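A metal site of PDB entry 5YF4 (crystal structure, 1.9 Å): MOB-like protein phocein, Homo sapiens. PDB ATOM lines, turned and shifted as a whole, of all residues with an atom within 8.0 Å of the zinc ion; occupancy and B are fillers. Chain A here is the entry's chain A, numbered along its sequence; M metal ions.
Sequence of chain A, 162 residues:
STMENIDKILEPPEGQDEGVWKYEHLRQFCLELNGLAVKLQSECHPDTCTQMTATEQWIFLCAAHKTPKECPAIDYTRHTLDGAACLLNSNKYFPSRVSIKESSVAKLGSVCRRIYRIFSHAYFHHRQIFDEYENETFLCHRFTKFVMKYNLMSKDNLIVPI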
ATOM      1  N   LEU A  40       0.752 -28.153  26.822  1.00  0.00           N
ATOM      2  CA  LEU A  40       1.517 -27.286  25.912  1.00  0.00           C
ATOM      3  C   LEU A  40       0.662 -26.199  25.280  1.00  0.00           C
ATOM      4  O   LEU A  40       1.170 -25.111  24.971  1.00  0.00           O
ATOM      5  CB  LEU A  40       2.149 -28.124  24.805  1.00  0.00           C
ATOM      6  CG  LEU A  40       3.264 -29.020  25.328  1.00  0.00           C
ATOM      7  CD1 LEU A  40       3.659 -29.917  24.209  1.00  0.00           C
ATOM      8  CD2 LEU A  40       4.440 -28.164  25.746  1.00  0.00           C
ATOM      9  N   GLN A  41      -0.627 -26.491  25.028  1.00  0.00           N
ATOM     10  CA  GLN A  41      -1.376 -25.531  24.226  1.00  0.00           C
ATOM     11  C   GLN A  41      -1.609 -24.217  24.967  1.00  0.00           C
ATOM     12  O   GLN A  41      -2.099 -23.247  24.358  1.00  0.00           O
ATOM     13  CB  GLN A  41      -2.684 -26.138  23.768  1.00  0.00           C
ATOM     14  CG  GLN A  41      -3.666 -26.356  24.841  1.00  0.00           C
ATOM     15  CD  GLN A  41      -4.835 -27.216  24.381  1.00  0.00           C
ATOM     16  OE1 GLN A  41      -4.725 -27.978  23.410  1.00  0.00           O
ATOM     17  NE2 GLN A  41      -5.968 -27.092  25.070  1.00  0.00           N
ATOM     18  N   GLU A  43       0.972 -22.405  26.055  1.00  0.00           N
ATOM     19  CA  GLU A  43       1.951 -21.441  25.568  1.00  0.00           C
ATOM     20  C   GLU A  43       2.516 -21.760  24.188  1.00  0.00           C
ATOM     21  O   GLU A  43       3.226 -20.929  23.641  1.00  0.00           O
ATOM     22  CB  GLU A  43       3.115 -21.260  26.550  1.00  0.00           C
ATOM     23  CG  GLU A  43       3.847 -22.514  26.840  1.00  0.00           C
ATOM     24  CD  GLU A  43       5.056 -22.340  27.772  1.00  0.00           C
ATOM     25  OE1 GLU A  43       6.114 -22.934  27.462  1.00  0.00           O
ATOM     26  OE2 GLU A  43       4.931 -21.678  28.827  1.00  0.00           O
ATOM     27  N   CYS A  44       2.208 -22.910  23.616  1.00  0.00           N
ATOM     28  CA  CYS A  44       2.728 -23.239  22.271  1.00  0.00           C
ATOM     29  C   CYS A  44       1.657 -22.757  21.306  1.00  0.00           C
ATOM     30  O   CYS A  44       0.671 -23.449  21.066  1.00  0.00           O
ATOM     31  CB  CYS A  44       2.947 -24.742  22.135  1.00  0.00           C
ATOM     32  SG  CYS A  44       3.591 -25.173  20.510  1.00  0.00           S
ATOM     33  N   HIS A  45       1.813 -21.549  20.803  1.00  0.00           N
ATOM     34  CA  HIS A  45       0.876 -20.846  19.889  1.00  0.00           C
ATOM     35  C   HIS A  45       1.430 -20.612  18.511  1.00  0.00           C
ATOM     36  O   HIS A  45       2.571 -20.425  18.375  1.00  0.00           O
ATOM     37  CB  HIS A  45       0.425 -19.517  20.483  1.00  0.00           C
ATOM     38  CG  HIS A  45      -0.376 -19.680  21.730  1.00  0.00           C
ATOM     39  ND1 HIS A  45      -0.331 -18.789  22.744  1.00  0.00           N
ATOM     40  CD2 HIS A  45      -1.208 -20.654  22.133  1.00  0.00           C
ATOM     41  CE1 HIS A  45      -1.120 -19.177  23.724  1.00  0.00           C
ATOM     42  NE2 HIS A  45      -1.667 -20.313  23.380  1.00  0.00           N
ATOM     43  N   PRO A  46       0.563 -20.549  17.518  1.00  0.00           N
ATOM     44  CA  PRO A  46       1.093 -20.505  16.156  1.00  0.00           C
ATOM     45  C   PRO A  46       1.708 -19.163  15.785  1.00  0.00           C
ATOM     46  O   PRO A  46       2.386 -19.108  14.754  1.00  0.00           O
ATOM     47  CB  PRO A  46      -0.132 -20.863  15.273  1.00  0.00           C
ATOM     48  CG  PRO A  46      -1.310 -20.604  16.113  1.00  0.00           C
ATOM     49  CD  PRO A  46      -0.882 -20.816  17.552  1.00  0.00           C
ATOM     50  N   THR A  48       4.071 -17.791  17.614  1.00  0.00           N
ATOM     51  CA  THR A  48       5.468 -17.861  18.071  1.00  0.00           C
ATOM     52  C   THR A  48       6.109 -19.203  17.742  1.00  0.00           C
ATOM     53  O   THR A  48       7.231 -19.230  17.219  1.00  0.00           O
ATOM     54  CB  THR A  48       5.573 -17.580  19.576  1.00  0.00           C
ATOM     55  OG1 THR A  48       4.547 -18.305  20.251  1.00  0.00           O
ATOM     56  CG2 THR A  48       5.418 -16.107  19.864  1.00  0.00           C
ATOM     57  N   CYS A  49       5.409 -20.315  17.971  1.00  0.00           N
ATOM     58  CA  CYS A  49       5.863 -21.621  17.438  1.00  0.00           C
ATOM     59  C   CYS A  49       5.214 -21.823  16.068  1.00  0.00           C
ATOM     60  O   CYS A  49       4.254 -22.568  15.897  1.00  0.00           O
ATOM     61  CB  CYS A  49       5.536 -22.740  18.418  1.00  0.00           C
ATOM     62  SG  CYS A  49       6.625 -22.742  19.886  1.00  0.00           S
ATOM     63  N   THR A  50       5.770 -21.135  15.057  1.00  0.00           N
ATOM     64  CA  THR A  50       5.165 -21.088  13.729  1.00  0.00           C
ATOM     65  C   THR A  50       5.459 -22.344  12.919  1.00  0.00           C
ATOM     66  O   THR A  50       4.805 -22.570  11.893  1.00  0.00           O
ATOM     67  CB  THR A  50       5.713 -19.905  12.955  1.00  0.00           C
ATOM     68  OG1 THR A  50       7.114 -20.140  12.762  1.00  0.00           O
ATOM     69  CG2 THR A  50       5.537 -18.558  13.726  1.00  0.00           C
ATOM     70  N   GLN A  51       6.407 -23.166  13.359  1.00  0.00           N
ATOM     71  CA  GLN A  51       6.796 -24.403  12.710  1.00  0.00           C
ATOM     72  C   GLN A  51       7.046 -25.511  13.726  1.00  0.00           C
ATOM     73  O   GLN A  51       7.251 -25.241  14.835  1.00  0.00           O
ATOM     74  CB  GLN A  51       8.074 -24.240  11.958  1.00  0.00           C
ATOM     75  CG  GLN A  51       8.051 -23.153  10.909  1.00  0.00           C
ATOM     76  CD  GLN A  51       9.420 -22.835  10.317  1.00  0.00           C
ATOM     77  OE1 GLN A  51       9.581 -22.886   9.150  1.00  0.00           O
ATOM     78  NE2 GLN A  51      10.355 -22.498  11.140  1.00  0.00           N
ATOM     79  N   MET A  52       7.081 -26.735  13.264  1.00  0.00           N
ATOM     80  CA  MET A  52       7.389 -27.848  14.166  1.00  0.00           C
ATOM     81  C   MET A  52       8.917 -28.048  14.102  1.00  0.00           C
ATOM     82  O   MET A  52       9.437 -28.511  13.087  1.00  0.00           O
ATOM     83  CB  MET A  52       6.658 -29.146  13.785  1.00  0.00           C
ATOM     84  CG  MET A  52       7.054 -30.204  14.797  1.00  0.00           C
ATOM     85  SD  MET A  52       6.267 -29.760  16.415  1.00  0.00           S
ATOM     86  CE  MET A  52       5.923 -31.362  17.161  1.00  0.00           C
ATOM     87  N   THR A  53       9.646 -27.642  15.156  1.00  0.00           N
ATOM     88  CA  THR A  53      11.094 -27.885  15.198  1.00  0.00           C
ATOM     89  C   THR A  53      11.504 -28.417  16.563  1.00  0.00           C
ATOM     90  O   THR A  53      10.750 -28.340  17.531  1.00  0.00           O
ATOM     91  CB  THR A  53      11.921 -26.618  14.907  1.00  0.00           C
ATOM     92  OG1 THR A  53      11.680 -25.638  15.932  1.00  0.00           O
ATOM     93  CG2 THR A  53      11.559 -25.982  13.509  1.00  0.00           C
ATOM     94  N   PRO A  72       2.072 -25.191  12.171  1.00  0.00           N
ATOM     95  CA  PRO A  72       2.646 -24.711  13.432  1.00  0.00           C
ATOM     96  C   PRO A  72       2.707 -25.852  14.415  1.00  0.00           C
ATOM     97  O   PRO A  72       1.963 -26.843  14.319  1.00  0.00           O
ATOM     98  CB  PRO A  72       1.637 -23.645  13.905  1.00  0.00           C
ATOM     99  CG  PRO A  72       0.777 -23.357  12.733  1.00  0.00           C
ATOM    100  CD  PRO A  72       0.765 -24.591  11.883  1.00  0.00           C
ATOM    101  N   ALA A  73       3.582 -25.703  15.423  1.00  0.00           N
ATOM    102  CA  ALA A  73       3.867 -26.829  16.308  1.00  0.00           C
ATOM    103  C   ALA A  73       2.608 -27.373  16.982  1.00  0.00           C
ATOM    104  O   ALA A  73       2.468 -28.599  17.132  1.00  0.00           O
ATOM    105  CB  ALA A  73       4.873 -26.437  17.388  1.00  0.00           C
ATOM    106  N   ILE A  74       1.733 -26.490  17.377  1.00  0.00           N
ATOM    107  CA  ILE A  74       0.534 -26.916  18.062  1.00  0.00           C
ATOM    108  C   ILE A  74      -0.357 -27.752  17.156  1.00  0.00           C
ATOM    109  O   ILE A  74      -0.948 -28.659  17.581  1.00  0.00           O
ATOM    110  CB  ILE A  74      -0.183 -25.736  18.760  1.00  0.00           C
ATOM    111  CG1 ILE A  74      -0.978 -26.213  19.958  1.00  0.00           C
ATOM    112  CG2 ILE A  74      -0.903 -24.839  17.812  1.00  0.00           C
ATOM    113  CD1 ILE A  74      -2.450 -26.336  19.719  1.00  0.00           C
ATOM    114  N   THR A  77       1.302 -31.169  16.517  1.00  0.00           N
ATOM    115  CA  THR A  77       1.052 -32.015  17.690  1.00  0.00           C
ATOM    116  C   THR A  77      -0.339 -32.635  17.652  1.00  0.00           C
ATOM    117  O   THR A  77      -0.497 -33.854  17.762  1.00  0.00           O
ATOM    118  CB  THR A  77       1.271 -31.185  18.950  1.00  0.00           C
ATOM    119  OG1 THR A  77       2.664 -30.826  18.973  1.00  0.00           O
ATOM    120  CG2 THR A  77       0.965 -31.993  20.212  1.00  0.00           C
ATOM    121  N   HIS A 121      10.071 -31.256  20.648  1.00  0.00           N
ATOM    122  CA  HIS A 121       9.664 -29.854  20.595  1.00  0.00           C
ATOM    123  C   HIS A 121       9.420 -29.319  21.999  1.00  0.00           C
ATOM    124  O   HIS A 121       9.809 -28.186  22.330  1.00  0.00           O
ATOM    125  CB  HIS A 121       8.385 -29.655  19.735  1.00  0.00           C
ATOM    126  CG  HIS A 121       7.926 -28.221  19.713  1.00  0.00           C
ATOM    127  ND1 HIS A 121       8.567 -27.251  18.975  1.00  0.00           N
ATOM    128  CD2 HIS A 121       6.936 -27.580  20.395  1.00  0.00           C
ATOM    129  CE1 HIS A 121       7.977 -26.075  19.180  1.00  0.00           C
ATOM    130  NE2 HIS A 121       6.965 -26.240  20.007  1.00  0.00           N
ATOM    131  N   ALA A 122       8.750 -30.086  22.844  1.00  0.00           N
ATOM    132  CA  ALA A 122       8.496 -29.589  24.184  1.00  0.00           C
ATOM    133  C   ALA A 122       9.810 -29.461  24.963  1.00  0.00           C
ATOM    134  O   ALA A 122       9.989 -28.515  25.731  1.00  0.00           O
ATOM    135  CB  ALA A 122       7.559 -30.530  24.933  1.00  0.00           C
ATOM    136  N   PHE A 124      12.873 -28.856  23.964  1.00  0.00           N
ATOM    137  CA  PHE A 124      13.757 -27.750  23.584  1.00  0.00           C
ATOM    138  C   PHE A 124      13.086 -26.402  23.583  1.00  0.00           C
ATOM    139  O   PHE A 124      13.773 -25.409  23.817  1.00  0.00           O
ATOM    140  CB  PHE A 124      14.394 -28.041  22.232  1.00  0.00           C
ATOM    141  CG  PHE A 124      15.380 -29.199  22.285  1.00  0.00           C
ATOM    142  CD1 PHE A 124      15.093 -30.410  21.664  1.00  0.00           C
ATOM    143  CD2 PHE A 124      16.588 -29.079  23.004  1.00  0.00           C
ATOM    144  CE1 PHE A 124      16.010 -31.503  21.746  1.00  0.00           C
ATOM    145  CE2 PHE A 124      17.505 -30.152  23.077  1.00  0.00           C
ATOM    146  CZ  PHE A 124      17.203 -31.353  22.434  1.00  0.00           C
ATOM    147  N   HIS A 125      11.778 -26.322  23.333  1.00  0.00           N
ATOM    148  CA  HIS A 125      11.120 -25.019  23.241  1.00  0.00           C
ATOM    149  C   HIS A 125      10.139 -24.748  24.371  1.00  0.00           C
ATOM    150  O   HIS A 125       9.645 -23.621  24.474  1.00  0.00           O
ATOM    151  CB  HIS A 125      10.408 -24.852  21.900  1.00  0.00           C
ATOM    152  CG  HIS A 125      11.336 -24.979  20.724  1.00  0.00           C
ATOM    153  ND1 HIS A 125      12.039 -23.907  20.214  1.00  0.00           N
ATOM    154  CD2 HIS A 125      11.757 -26.072  20.034  1.00  0.00           C
ATOM    155  CE1 HIS A 125      12.811 -24.315  19.226  1.00  0.00           C
ATOM    156  NE2 HIS A 125      12.670 -25.631  19.103  1.00  0.00           N
ATOM    157  N   HIS A 126       9.858 -25.737  25.232  1.00  0.00           N
ATOM    158  CA  HIS A 126       8.934 -25.556  26.376  1.00  0.00           C
ATOM    159  C   HIS A 126       9.483 -26.309  27.589  1.00  0.00           C
ATOM    160  O   HIS A 126       8.797 -27.112  28.222  1.00  0.00           O
ATOM    161  CB  HIS A 126       7.538 -26.051  25.998  1.00  0.00           C
ATOM    162  CG  HIS A 126       6.953 -25.347  24.787  1.00  0.00           C
ATOM    163  ND1 HIS A 126       6.488 -24.051  24.816  1.00  0.00           N
ATOM    164  CD2 HIS A 126       6.818 -25.772  23.501  1.00  0.00           C
ATOM    165  CE1 HIS A 126       6.079 -23.711  23.593  1.00  0.00           C
ATOM    166  NE2 HIS A 126       6.257 -24.737  22.797  1.00  0.00           N
HETATM  167 ZN    ZN M   1       5.815 -24.715  20.817  1.00  0.00          ZN
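The zinc ion is bound by a ring nitrogen (NE2) of His 126 (2.0 Å), a ring nitrogen (NE2) of His 121 (2.1 Å), the side-chain sulfur of Cys 44 (2.3 Å) and the side-chain sulfur of Cys 49 (2.3 Å).
Residues that only touch the zinc ion: Ala 73. Within 4 Å of the zinc ion: Cys 44, Cys 49, Ala 73, His 121 and His 126.
The backbone carbonyl oxygen of Thr 53 lies within hydrogen-bond range of a ring nitrogen (ND1) of His 121 (2.8 Å). N of Ala 73 sits at hydrogen-bond distance from O of Cys 49, 3.2 Å away. The backbone carbonyl oxygen of Ala 73 is in hydrogen-bond range of the side-chain hydroxyl of Thr 77 (2.9 Å). The side-chain carboxylate (OE1) of Glu 43 lies within hydrogen-bond range of a ring nitrogen (ND1) of His 126.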
